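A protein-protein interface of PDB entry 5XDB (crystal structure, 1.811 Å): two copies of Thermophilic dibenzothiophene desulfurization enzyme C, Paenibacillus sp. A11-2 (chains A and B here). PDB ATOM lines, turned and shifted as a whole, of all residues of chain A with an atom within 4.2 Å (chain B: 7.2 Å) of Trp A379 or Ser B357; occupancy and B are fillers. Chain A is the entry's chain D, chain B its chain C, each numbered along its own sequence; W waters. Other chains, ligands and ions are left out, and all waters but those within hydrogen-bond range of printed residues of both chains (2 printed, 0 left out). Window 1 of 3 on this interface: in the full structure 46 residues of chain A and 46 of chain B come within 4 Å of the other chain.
Among the printed residues, merely in contact across the chains: Leu A205 with Tyr B360 (3.6 Å), Leu A205 with Asp B376 (3.4 Å), Ile A353 with Ser B357 (3.5 Å), Asp A376 with Trp B379 (3.98 Å), Trp A379 with Tyr B360 (3.9 Å), Trp A379 with Asp B376 (3.99 Å), Trp A379 with Trp B379 (3.5 Å), Arg A383 with Arg B358 (3.96 Å) and Arg A383 with Tyr B360 (3.6 Å).
Asp A376 touches Trp B379, and with the chains exchanged Trp A379 touches Asp B376. Trp A379 touches its own counterpart, Trp B379. Of the 12 pairs that touch across the chains among the printed residues, 3 have their exchanged pair printed and touching as well.
Of the printed residues of chain B, Trp A379 touches Ser B357, Tyr B360, Asp B376 and Trp B379. Of chain A, only Ile A353, Trp A379 and Arg A383 come within 4 Å of Ser B357. Of the printed residues of chain A, Arg B358 touches Arg A383. Printed residues of chain A within 4 Å of Trp B379: Asp A376 and Trp A379. Of the printed residues of chain B, Leu A205 touches Tyr B360 (3.6 Å) and Asp B376 (3.4 Å). Printed residues of chain B within 4 Å of Asp A376: Trp B379. The nearest printed residue of chain A that does not touch Ser B357 is Thr A356 (6.4 Å). The nearest printed residue of chain B that does not touch Arg A383 is Leu B359 (5.4 Å).
The backbone NH (N) of Asp B376 lies within hydrogen-bond range of the side-chain hydroxyl (OH) of Tyr B360 (3.1 Å). NE of Arg B358 lies within salt-bridge range of OE2 of Glu B361 (2.8 Å). NE of Arg A380 is in salt-bridge range of OD2 of Asp A376. O of Ile A353 is in hydrogen-bond range of OG1 of Thr A356 (3.5 Å). The backbone carbonyl oxygen of Leu A205 lies within hydrogen-bond range of the guanidinium group of Arg A380, at 3.0 Å. OD2 of Asp B376 lies within salt-bridge range of NE of Arg B380 (2.8 Å).
Water W2 lies within hydrogen-bond range of the backbone carbonyl oxygen of Ile A353 (2.8 Å) and the side-chain hydroxyl of Ser B357 (2.8 Å). Water W1 lies within hydrogen-bond range of NH2 of Arg A383 (2.8 Å) and OE2 of Glu B361 (3.4 Å).
Hydrophobic or aromatic side chains of chain B that line the printed part of chain A: Tyr B360 and Trp B379. Of the 11 printed residues of chain A, 5 touch a printed residue of chain B. Printed residues of chain A that touch a printed residue of chain B: Leu A205, Ile A353, Asp A376, Trp A379 and Arg A383.
NH1 of Arg A383 is in salt-bridge range of OE2 of Glu B361, 3.0 Å away. NE1 of Trp A379 is in hydrogen-bond range of OG of Ser B357 (3.0 Å). The backbone carbonyl oxygen of Ser B357 lies within hydrogen-bond range of the guanidinium group of Arg A383.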
ATOM      1  N   LEU A 205     -30.012  27.984  31.517  1.00  0.00           N
ATOM      2  CA  LEU A 205     -28.621  27.956  31.075  1.00  0.00           C
ATOM      3  C   LEU A 205     -28.228  29.274  30.419  1.00  0.00           C
ATOM      4  O   LEU A 205     -27.227  29.898  30.789  1.00  0.00           O
ATOM      5  CB  LEU A 205     -28.419  26.795  30.107  1.00  0.00           C
ATOM      6  CG  LEU A 205     -27.053  26.699  29.419  1.00  0.00           C
ATOM      7  CD1 LEU A 205     -25.934  26.492  30.454  1.00  0.00           C
ATOM      8  CD2 LEU A 205     -27.095  25.575  28.387  1.00  0.00           C
ATOM      9  N   ILE A 353     -24.774  27.681  16.524  1.00  0.00           N
ATOM     10  CA  ILE A 353     -24.376  26.616  17.446  1.00  0.00           C
ATOM     11  C   ILE A 353     -22.930  26.190  17.189  1.00  0.00           C
ATOM     12  O   ILE A 353     -22.168  25.934  18.129  1.00  0.00           O
ATOM     13  CB  ILE A 353     -25.356  25.436  17.334  1.00  0.00           C
ATOM     14  CG1 ILE A 353     -26.746  25.875  17.804  1.00  0.00           C
ATOM     15  CG2 ILE A 353     -24.870  24.237  18.157  1.00  0.00           C
ATOM     16  CD1 ILE A 353     -26.744  26.345  19.264  1.00  0.00           C
ATOM     17  N   THR A 356     -20.317  29.427  18.069  1.00  0.00           N
ATOM     18  CA  THR A 356     -20.177  29.830  19.471  1.00  0.00           C
ATOM     19  C   THR A 356     -19.337  28.835  20.265  1.00  0.00           C
ATOM     20  O   THR A 356     -18.755  29.205  21.289  1.00  0.00           O
ATOM     21  CB  THR A 356     -21.546  30.032  20.146  1.00  0.00           C
ATOM     22  OG1 THR A 356     -22.336  28.846  20.054  1.00  0.00           O
ATOM     23  CG2 THR A 356     -22.289  31.204  19.509  1.00  0.00           C
ATOM     24  N   ASP A 376     -18.597  32.111  26.972  1.00  0.00           N
ATOM     25  CA  ASP A 376     -19.560  31.022  26.893  1.00  0.00           C
ATOM     26  C   ASP A 376     -20.995  31.525  26.908  1.00  0.00           C
ATOM     27  O   ASP A 376     -21.903  30.758  26.573  1.00  0.00           O
ATOM     28  CB  ASP A 376     -19.328  30.036  28.041  1.00  0.00           C
ATOM     29  CG  ASP A 376     -19.518  30.673  29.406  1.00  0.00           C
ATOM     30  OD1 ASP A 376     -18.738  31.591  29.743  1.00  0.00           O
ATOM     31  OD2 ASP A 376     -20.447  30.267  30.128  1.00  0.00           O
ATOM     32  N   ARG A 377     -21.219  32.793  27.275  1.00  0.00           N
ATOM     33  CA  ARG A 377     -22.567  33.350  27.220  1.00  0.00           C
ATOM     34  C   ARG A 377     -23.193  33.160  25.839  1.00  0.00           C
ATOM     35  O   ARG A 377     -24.388  32.863  25.727  1.00  0.00           O
ATOM     36  CB  ARG A 377     -22.516  34.834  27.601  1.00  0.00           C
ATOM     37  CG  ARG A 377     -23.854  35.570  27.538  1.00  0.00           C
ATOM     38  CD  ARG A 377     -23.700  36.994  28.102  1.00  0.00           C
ATOM     39  NE  ARG A 377     -22.647  37.728  27.399  1.00  0.00           N
ATOM     40  CZ  ARG A 377     -22.832  38.408  26.268  1.00  0.00           C
ATOM     41  NH1 ARG A 377     -24.042  38.479  25.706  1.00  0.00           N
ATOM     42  NH2 ARG A 377     -21.806  39.027  25.703  1.00  0.00           N
ATOM     43  N   PHE A 378     -22.402  33.324  24.773  1.00  0.00           N
ATOM     44  CA  PHE A 378     -22.958  33.220  23.428  1.00  0.00           C
ATOM     45  C   PHE A 378     -23.470  31.808  23.161  1.00  0.00           C
ATOM     46  O   PHE A 378     -24.610  31.621  22.724  1.00  0.00           O
ATOM     47  CB  PHE A 378     -21.913  33.637  22.390  1.00  0.00           C
ATOM     48  CG  PHE A 378     -21.490  35.091  22.499  1.00  0.00           C
ATOM     49  CD1 PHE A 378     -22.280  36.102  21.965  1.00  0.00           C
ATOM     50  CD2 PHE A 378     -20.295  35.437  23.128  1.00  0.00           C
ATOM     51  CE1 PHE A 378     -21.901  37.445  22.064  1.00  0.00           C
ATOM     52  CE2 PHE A 378     -19.899  36.783  23.230  1.00  0.00           C
ATOM     53  CZ  PHE A 378     -20.703  37.777  22.691  1.00  0.00           C
ATOM     54  N   TRP A 379     -22.646  30.797  23.441  1.00  0.00           N
ATOM     55  CA  TRP A 379     -23.115  29.423  23.285  1.00  0.00           C
ATOM     56  C   TRP A 379     -24.311  29.144  24.198  1.00  0.00           C
ATOM     57  O   TRP A 379     -25.311  28.553  23.768  1.00  0.00           O
ATOM     58  CB  TRP A 379     -21.973  28.439  23.554  1.00  0.00           C
ATOM     59  CG  TRP A 379     -22.428  26.987  23.517  1.00  0.00           C
ATOM     60  CD1 TRP A 379     -22.553  26.187  22.409  1.00  0.00           C
ATOM     61  CD2 TRP A 379     -22.829  26.188  24.639  1.00  0.00           C
ATOM     62  NE1 TRP A 379     -23.015  24.940  22.777  1.00  0.00           N
ATOM     63  CE2 TRP A 379     -23.175  24.910  24.141  1.00  0.00           C
ATOM     64  CE3 TRP A 379     -22.910  26.422  26.017  1.00  0.00           C
ATOM     65  CZ2 TRP A 379     -23.605  23.870  24.974  1.00  0.00           C
ATOM     66  CZ3 TRP A 379     -23.359  25.400  26.843  1.00  0.00           C
ATOM     67  CH2 TRP A 379     -23.696  24.132  26.316  1.00  0.00           C
ATOM     68  N   ARG A 380     -24.251  29.588  25.454  1.00  0.00           N
ATOM     69  CA  ARG A 380     -25.365  29.307  26.359  1.00  0.00           C
ATOM     70  C   ARG A 380     -26.666  29.922  25.841  1.00  0.00           C
ATOM     71  O   ARG A 380     -27.715  29.265  25.820  1.00  0.00           O
ATOM     72  CB  ARG A 380     -25.046  29.807  27.768  1.00  0.00           C
ATOM     73  CG  ARG A 380     -24.008  28.964  28.512  1.00  0.00           C
ATOM     74  CD  ARG A 380     -23.887  29.385  29.994  1.00  0.00           C
ATOM     75  NE  ARG A 380     -23.169  30.645  30.192  1.00  0.00           N
ATOM     76  CZ  ARG A 380     -23.733  31.822  30.465  1.00  0.00           C
ATOM     77  NH1 ARG A 380     -25.057  31.944  30.554  1.00  0.00           N
ATOM     78  NH2 ARG A 380     -22.975  32.897  30.644  1.00  0.00           N
ATOM     79  N   ASP A 381     -26.615  31.180  25.409  1.00  0.00           N
ATOM     80  CA  ASP A 381     -27.816  31.826  24.880  1.00  0.00           C
ATOM     81  C   ASP A 381     -28.315  31.113  23.626  1.00  0.00           C
ATOM     82  O   ASP A 381     -29.512  30.818  23.495  1.00  0.00           O
ATOM     83  CB  ASP A 381     -27.529  33.300  24.556  1.00  0.00           C
ATOM     84  CG  ASP A 381     -27.245  34.145  25.786  1.00  0.00           C
ATOM     85  OD1 ASP A 381     -27.675  33.773  26.905  1.00  0.00           O
ATOM     86  OD2 ASP A 381     -26.611  35.206  25.589  1.00  0.00           O
ATOM     87  N   ALA A 382     -27.411  30.854  22.675  1.00  0.00           N
ATOM     88  CA  ALA A 382     -27.808  30.205  21.433  1.00  0.00           C
ATOM     89  C   ALA A 382     -28.283  28.778  21.697  1.00  0.00           C
ATOM     90  O   ALA A 382     -29.333  28.356  21.201  1.00  0.00           O
ATOM     91  CB  ALA A 382     -26.648  30.219  20.432  1.00  0.00           C
ATOM     92  N   ARG A 383     -27.537  28.031  22.509  1.00  0.00           N
ATOM     93  CA  ARG A 383     -27.911  26.643  22.758  1.00  0.00           C
ATOM     94  C   ARG A 383     -29.285  26.555  23.402  1.00  0.00           C
ATOM     95  O   ARG A 383     -30.048  25.619  23.126  1.00  0.00           O
ATOM     96  CB  ARG A 383     -26.867  25.961  23.642  1.00  0.00           C
ATOM     97  CG  ARG A 383     -27.179  24.497  23.962  1.00  0.00           C
ATOM     98  CD  ARG A 383     -27.149  23.559  22.736  1.00  0.00           C
ATOM     99  NE  ARG A 383     -28.262  23.782  21.808  1.00  0.00           N
ATOM    100  CZ  ARG A 383     -28.409  23.143  20.648  1.00  0.00           C
ATOM    101  NH1 ARG A 383     -27.522  22.215  20.280  1.00  0.00           N
ATOM    102  NH2 ARG A 383     -29.438  23.437  19.845  1.00  0.00           N
ATOM    103  N   PHE B 302     -23.549   9.649  17.320  1.00  0.00           N
ATOM    104  CA  PHE B 302     -22.511   9.881  18.314  1.00  0.00           C
ATOM    105  C   PHE B 302     -22.077   8.590  18.999  1.00  0.00           C
ATOM    106  O   PHE B 302     -20.882   8.408  19.264  1.00  0.00           O
ATOM    107  CB  PHE B 302     -22.989  10.934  19.319  1.00  0.00           C
ATOM    108  CG  PHE B 302     -23.027  12.324  18.735  1.00  0.00           C
ATOM    109  CD1 PHE B 302     -21.918  12.838  18.081  1.00  0.00           C
ATOM    110  CD2 PHE B 302     -24.178  13.091  18.799  1.00  0.00           C
ATOM    111  CE1 PHE B 302     -21.945  14.115  17.522  1.00  0.00           C
ATOM    112  CE2 PHE B 302     -24.221  14.364  18.241  1.00  0.00           C
ATOM    113  CZ  PHE B 302     -23.103  14.876  17.593  1.00  0.00           C
ATOM    114  N   LEU B 351     -15.250  14.754  18.364  1.00  0.00           N
ATOM    115  CA  LEU B 351     -16.402  14.017  18.869  1.00  0.00           C
ATOM    116  C   LEU B 351     -16.961  14.663  20.125  1.00  0.00           C
ATOM    117  O   LEU B 351     -18.161  14.952  20.206  1.00  0.00           O
ATOM    118  CB  LEU B 351     -16.012  12.560  19.139  1.00  0.00           C
ATOM    119  CG  LEU B 351     -17.061  11.723  19.864  1.00  0.00           C
ATOM    120  CD1 LEU B 351     -18.338  11.675  18.999  1.00  0.00           C
ATOM    121  CD2 LEU B 351     -16.542  10.319  20.198  1.00  0.00           C
ATOM    122  N   VAL B 352     -16.116  14.868  21.140  1.00  0.00           N
ATOM    123  CA  VAL B 352     -16.649  15.351  22.411  1.00  0.00           C
ATOM    124  C   VAL B 352     -17.182  16.775  22.275  1.00  0.00           C
ATOM    125  O   VAL B 352     -18.199  17.123  22.881  1.00  0.00           O
ATOM    126  CB  VAL B 352     -15.596  15.237  23.526  1.00  0.00           C
ATOM    127  CG1 VAL B 352     -14.461  16.240  23.323  1.00  0.00           C
ATOM    128  CG2 VAL B 352     -16.282  15.424  24.891  1.00  0.00           C
ATOM    129  N   ILE B 353     -16.526  17.617  21.472  1.00  0.00           N
ATOM    130  CA  ILE B 353     -17.011  18.990  21.320  1.00  0.00           C
ATOM    131  C   ILE B 353     -18.367  19.014  20.615  1.00  0.00           C
ATOM    132  O   ILE B 353     -19.259  19.784  20.991  1.00  0.00           O
ATOM    133  CB  ILE B 353     -15.975  19.857  20.585  1.00  0.00           C
ATOM    134  CG1 ILE B 353     -14.745  20.046  21.468  1.00  0.00           C
ATOM    135  CG2 ILE B 353     -16.576  21.225  20.216  1.00  0.00           C
ATOM    136  CD1 ILE B 353     -15.050  20.696  22.828  1.00  0.00           C
ATOM    137  N   GLU B 354     -18.551  18.186  19.578  1.00  0.00           N
ATOM    138  CA  GLU B 354     -19.849  18.173  18.893  1.00  0.00           C
ATOM    139  C   GLU B 354     -20.926  17.565  19.772  1.00  0.00           C
ATOM    140  O   GLU B 354     -22.011  18.135  19.937  1.00  0.00           O
ATOM    141  CB  GLU B 354     -19.780  17.393  17.579  1.00  0.00           C
ATOM    142  CG  GLU B 354     -18.723  17.857  16.610  1.00  0.00           C
ATOM    143  CD  GLU B 354     -18.793  17.093  15.298  1.00  0.00           C
ATOM    144  OE1 GLU B 354     -18.066  17.464  14.347  1.00  0.00           O
ATOM    145  OE2 GLU B 354     -19.587  16.122  15.220  1.00  0.00           O
ATOM    146  N   LEU B 355     -20.646  16.393  20.332  1.00  0.00           N
ATOM    147  CA  LEU B 355     -21.647  15.657  21.097  1.00  0.00           C
ATOM    148  C   LEU B 355     -22.163  16.467  22.288  1.00  0.00           C
ATOM    149  O   LEU B 355     -23.376  16.522  22.532  1.00  0.00           O
ATOM    150  CB  LEU B 355     -21.020  14.329  21.535  1.00  0.00           C
ATOM    151  CG  LEU B 355     -21.604  13.315  22.495  1.00  0.00           C
ATOM    152  CD1 LEU B 355     -20.831  12.014  22.301  1.00  0.00           C
ATOM    153  CD2 LEU B 355     -21.453  13.812  23.910  1.00  0.00           C
ATOM    154  N   THR B 356     -21.267  17.127  23.031  1.00  0.00           N
ATOM    155  CA  THR B 356     -21.699  17.777  24.267  1.00  0.00           C
ATOM    156  C   THR B 356     -22.577  18.997  23.997  1.00  0.00           C
ATOM    157  O   THR B 356     -23.341  19.412  24.884  1.00  0.00           O
ATOM    158  CB  THR B 356     -20.487  18.166  25.137  1.00  0.00           C
ATOM    159  OG1 THR B 356     -19.610  19.037  24.419  1.00  0.00           O
ATOM    160  CG2 THR B 356     -19.720  16.910  25.561  1.00  0.00           C
ATOM    161  N   SER B 357     -22.499  19.563  22.799  1.00  0.00           N
ATOM    162  CA  SER B 357     -23.390  20.645  22.397  1.00  0.00           C
ATOM    163  C   SER B 357     -24.644  20.117  21.696  1.00  0.00           C
ATOM    164  O   SER B 357     -25.764  20.519  22.029  1.00  0.00           O
ATOM    165  CB  SER B 357     -22.635  21.626  21.491  1.00  0.00           C
ATOM    166  OG  SER B 357     -23.498  22.636  20.996  1.00  0.00           O
ATOM    167  N   ARG B 358     -24.484  19.195  20.743  1.00  0.00           N
ATOM    168  CA  ARG B 358     -25.611  18.766  19.916  1.00  0.00           C
ATOM    169  C   ARG B 358     -26.597  17.842  20.641  1.00  0.00           C
ATOM    170  O   ARG B 358     -27.756  17.760  20.225  1.00  0.00           O
ATOM    171  CB  ARG B 358     -25.097  18.071  18.647  1.00  0.00           C
ATOM    172  CG  ARG B 358     -24.221  18.942  17.735  1.00  0.00           C
ATOM    173  CD  ARG B 358     -25.008  19.749  16.692  1.00  0.00           C
ATOM    174  NE  ARG B 358     -26.262  19.110  16.273  1.00  0.00           N
ATOM    175  CZ  ARG B 358     -26.343  18.030  15.499  1.00  0.00           C
ATOM    176  NH1 ARG B 358     -25.238  17.439  15.054  1.00  0.00           N
ATOM    177  NH2 ARG B 358     -27.534  17.530  15.177  1.00  0.00           N
ATOM    178  N   LEU B 359     -26.184  17.152  21.717  1.00  0.00           N
ATOM    179  CA  LEU B 359     -27.132  16.287  22.414  1.00  0.00           C
ATOM    180  C   LEU B 359     -28.325  17.053  22.970  1.00  0.00           C
ATOM    181  O   LEU B 359     -29.380  16.451  23.166  1.00  0.00           O
ATOM    182  CB  LEU B 359     -26.444  15.510  23.544  1.00  0.00           C
ATOM    183  CG  LEU B 359     -25.756  14.223  23.067  1.00  0.00           C
ATOM    184  CD1 LEU B 359     -24.840  13.688  24.168  1.00  0.00           C
ATOM    185  CD2 LEU B 359     -26.767  13.164  22.681  1.00  0.00           C
ATOM    186  N   TYR B 360     -28.199  18.360  23.224  1.00  0.00           N
ATOM    187  CA  TYR B 360     -29.379  19.129  23.624  1.00  0.00           C
ATOM    188  C   TYR B 360     -30.524  18.950  22.633  1.00  0.00           C
ATOM    189  O   TYR B 360     -31.699  18.930  23.021  1.00  0.00           O
ATOM    190  CB  TYR B 360     -29.023  20.607  23.753  1.00  0.00           C
ATOM    191  CG  TYR B 360     -28.403  20.966  25.080  1.00  0.00           C
ATOM    192  CD1 TYR B 360     -29.205  21.240  26.189  1.00  0.00           C
ATOM    193  CD2 TYR B 360     -27.026  21.019  25.236  1.00  0.00           C
ATOM    194  CE1 TYR B 360     -28.655  21.573  27.420  1.00  0.00           C
ATOM    195  CE2 TYR B 360     -26.460  21.359  26.470  1.00  0.00           C
ATOM    196  CZ  TYR B 360     -27.279  21.632  27.550  1.00  0.00           C
ATOM    197  OH  TYR B 360     -26.734  21.964  28.768  1.00  0.00           O
ATOM    198  N   GLU B 361     -30.200  18.843  21.344  1.00  0.00           N
ATOM    199  CA  GLU B 361     -31.236  18.670  20.323  1.00  0.00           C
ATOM    200  C   GLU B 361     -31.972  17.346  20.453  1.00  0.00           C
ATOM    201  O   GLU B 361     -33.108  17.238  19.981  1.00  0.00           O
ATOM    202  CB  GLU B 361     -30.619  18.794  18.924  1.00  0.00           C
ATOM    203  CG  GLU B 361     -29.990  20.157  18.709  1.00  0.00           C
ATOM    204  CD  GLU B 361     -29.043  20.225  17.519  1.00  0.00           C
ATOM    205  OE1 GLU B 361     -29.409  19.683  16.451  1.00  0.00           O
ATOM    206  OE2 GLU B 361     -27.940  20.840  17.664  1.00  0.00           O
ATOM    207  N   ALA B 362     -31.360  16.334  21.080  1.00  0.00           N
ATOM    208  CA  ALA B 362     -32.050  15.088  21.386  1.00  0.00           C
ATOM    209  C   ALA B 362     -32.823  15.132  22.698  1.00  0.00           C
ATOM    210  O   ALA B 362     -33.585  14.198  22.982  1.00  0.00           O
ATOM    211  CB  ALA B 362     -31.050  13.927  21.440  1.00  0.00           C
ATOM    212  N   MET B 363     -32.621  16.161  23.520  1.00  0.00           N
ATOM    213  CA  MET B 363     -33.277  16.267  24.816  1.00  0.00           C
ATOM    214  C   MET B 363     -34.411  17.279  24.839  1.00  0.00           C
ATOM    215  O   MET B 363     -35.442  17.015  25.444  1.00  0.00           O
ATOM    216  CB  MET B 363     -32.252  16.625  25.904  1.00  0.00           C
ATOM    217  CG  MET B 363     -31.281  15.492  26.219  1.00  0.00           C
ATOM    218  SD  MET B 363     -30.166  15.890  27.578  1.00  0.00           S
ATOM    219  CE  MET B 363     -29.118  17.141  26.852  1.00  0.00           C
ATOM    220  N   PHE B 375     -26.337  19.919  32.553  1.00  0.00           N
ATOM    221  CA  PHE B 375     -25.741  19.118  31.481  1.00  0.00           C
ATOM    222  C   PHE B 375     -24.596  19.852  30.796  1.00  0.00           C
ATOM    223  O   PHE B 375     -23.705  19.211  30.223  1.00  0.00           O
ATOM    224  CB  PHE B 375     -26.805  18.717  30.454  1.00  0.00           C
ATOM    225  CG  PHE B 375     -26.298  17.774  29.384  1.00  0.00           C
ATOM    226  CD1 PHE B 375     -26.231  16.406  29.615  1.00  0.00           C
ATOM    227  CD2 PHE B 375     -25.891  18.264  28.142  1.00  0.00           C
ATOM    228  CE1 PHE B 375     -25.761  15.544  28.626  1.00  0.00           C
ATOM    229  CE2 PHE B 375     -25.423  17.415  27.149  1.00  0.00           C
ATOM    230  CZ  PHE B 375     -25.361  16.047  27.390  1.00  0.00           C
ATOM    231  N   ASP B 376     -24.609  21.185  30.831  1.00  0.00           N
ATOM    232  CA  ASP B 376     -23.571  21.981  30.191  1.00  0.00           C
ATOM    233  C   ASP B 376     -22.194  21.760  30.803  1.00  0.00           C
ATOM    234  O   ASP B 376     -21.195  22.195  30.215  1.00  0.00           O
ATOM    235  CB  ASP B 376     -23.943  23.464  30.277  1.00  0.00           C
ATOM    236  CG  ASP B 376     -24.044  23.949  31.706  1.00  0.00           C
ATOM    237  OD1 ASP B 376     -24.896  23.423  32.460  1.00  0.00           O
ATOM    238  OD2 ASP B 376     -23.275  24.859  32.074  1.00  0.00           O
ATOM    239  N   ARG B 377     -22.120  21.107  31.969  1.00  0.00           N
ATOM    240  CA  ARG B 377     -20.825  20.784  32.557  1.00  0.00           C
ATOM    241  C   ARG B 377     -19.964  20.000  31.578  1.00  0.00           C
ATOM    242  O   ARG B 377     -18.749  20.221  31.492  1.00  0.00           O
ATOM    243  CB  ARG B 377     -21.033  19.989  33.854  1.00  0.00           C
ATOM    244  CG  ARG B 377     -19.745  19.514  34.521  1.00  0.00           C
ATOM    245  CD  ARG B 377     -20.070  18.881  35.884  1.00  0.00           C
ATOM    246  NE  ARG B 377     -21.035  17.791  35.756  1.00  0.00           N
ATOM    247  CZ  ARG B 377     -20.725  16.531  35.480  1.00  0.00           C
ATOM    248  NH1 ARG B 377     -19.456  16.174  35.300  1.00  0.00           N
ATOM    249  NH2 ARG B 377     -21.687  15.622  35.378  1.00  0.00           N
ATOM    250  N   PHE B 378     -20.574  19.097  30.813  1.00  0.00           N
ATOM    251  CA  PHE B 378     -19.794  18.267  29.899  1.00  0.00           C
ATOM    252  C   PHE B 378     -19.152  19.115  28.806  1.00  0.00           C
ATOM    253  O   PHE B 378     -17.946  19.008  28.554  1.00  0.00           O
ATOM    254  CB  PHE B 378     -20.671  17.166  29.291  1.00  0.00           C
ATOM    255  CG  PHE B 378     -21.194  16.161  30.304  1.00  0.00           C
ATOM    256  CD1 PHE B 378     -20.376  15.136  30.776  1.00  0.00           C
ATOM    257  CD2 PHE B 378     -22.504  16.246  30.782  1.00  0.00           C
ATOM    258  CE1 PHE B 378     -20.851  14.209  31.696  1.00  0.00           C
ATOM    259  CE2 PHE B 378     -22.983  15.328  31.711  1.00  0.00           C
ATOM    260  CZ  PHE B 378     -22.148  14.307  32.174  1.00  0.00           C
ATOM    261  N   TRP B 379     -19.937  19.978  28.158  1.00  0.00           N
ATOM    262  CA  TRP B 379     -19.365  20.894  27.173  1.00  0.00           C
ATOM    263  C   TRP B 379     -18.329  21.815  27.810  1.00  0.00           C
ATOM    264  O   TRP B 379     -17.241  22.035  27.255  1.00  0.00           O
ATOM    265  CB  TRP B 379     -20.469  21.710  26.498  1.00  0.00           C
ATOM    266  CG  TRP B 379     -19.929  22.722  25.514  1.00  0.00           C
ATOM    267  CD1 TRP B 379     -19.583  22.497  24.199  1.00  0.00           C
ATOM    268  CD2 TRP B 379     -19.677  24.105  25.765  1.00  0.00           C
ATOM    269  NE1 TRP B 379     -19.121  23.669  23.629  1.00  0.00           N
ATOM    270  CE2 TRP B 379     -19.170  24.666  24.567  1.00  0.00           C
ATOM    271  CE3 TRP B 379     -19.824  24.929  26.887  1.00  0.00           C
ATOM    272  CZ2 TRP B 379     -18.811  26.003  24.466  1.00  0.00           C
ATOM    273  CZ3 TRP B 379     -19.477  26.260  26.785  1.00  0.00           C
ATOM    274  CH2 TRP B 379     -18.977  26.790  25.579  1.00  0.00           C
ATOM    275  N   ARG B 380     -18.643  22.377  28.975  1.00  0.00           N
ATOM    276  CA  ARG B 380     -17.687  23.290  29.602  1.00  0.00           C
ATOM    277  C   ARG B 380     -16.356  22.594  29.884  1.00  0.00           C
ATOM    278  O   ARG B 380     -15.288  23.150  29.604  1.00  0.00           O
ATOM    279  CB  ARG B 380     -18.266  23.872  30.890  1.00  0.00           C
ATOM    280  CG  ARG B 380     -19.355  24.937  30.667  1.00  0.00           C
ATOM    281  CD  ARG B 380     -19.779  25.642  31.997  1.00  0.00           C
ATOM    282  NE  ARG B 380     -20.614  24.810  32.866  1.00  0.00           N
ATOM    283  CZ  ARG B 380     -20.182  24.193  33.965  1.00  0.00           C
ATOM    284  NH1 ARG B 380     -18.906  24.298  34.342  1.00  0.00           N
ATOM    285  NH2 ARG B 380     -21.020  23.475  34.695  1.00  0.00           N
HETATM  286  O   HOH W   1     -30.484  23.044  17.259  1.00  0.00           O
HETATM  287  O   HOH W   2     -21.740  23.321  18.922  1.00  0.00           O
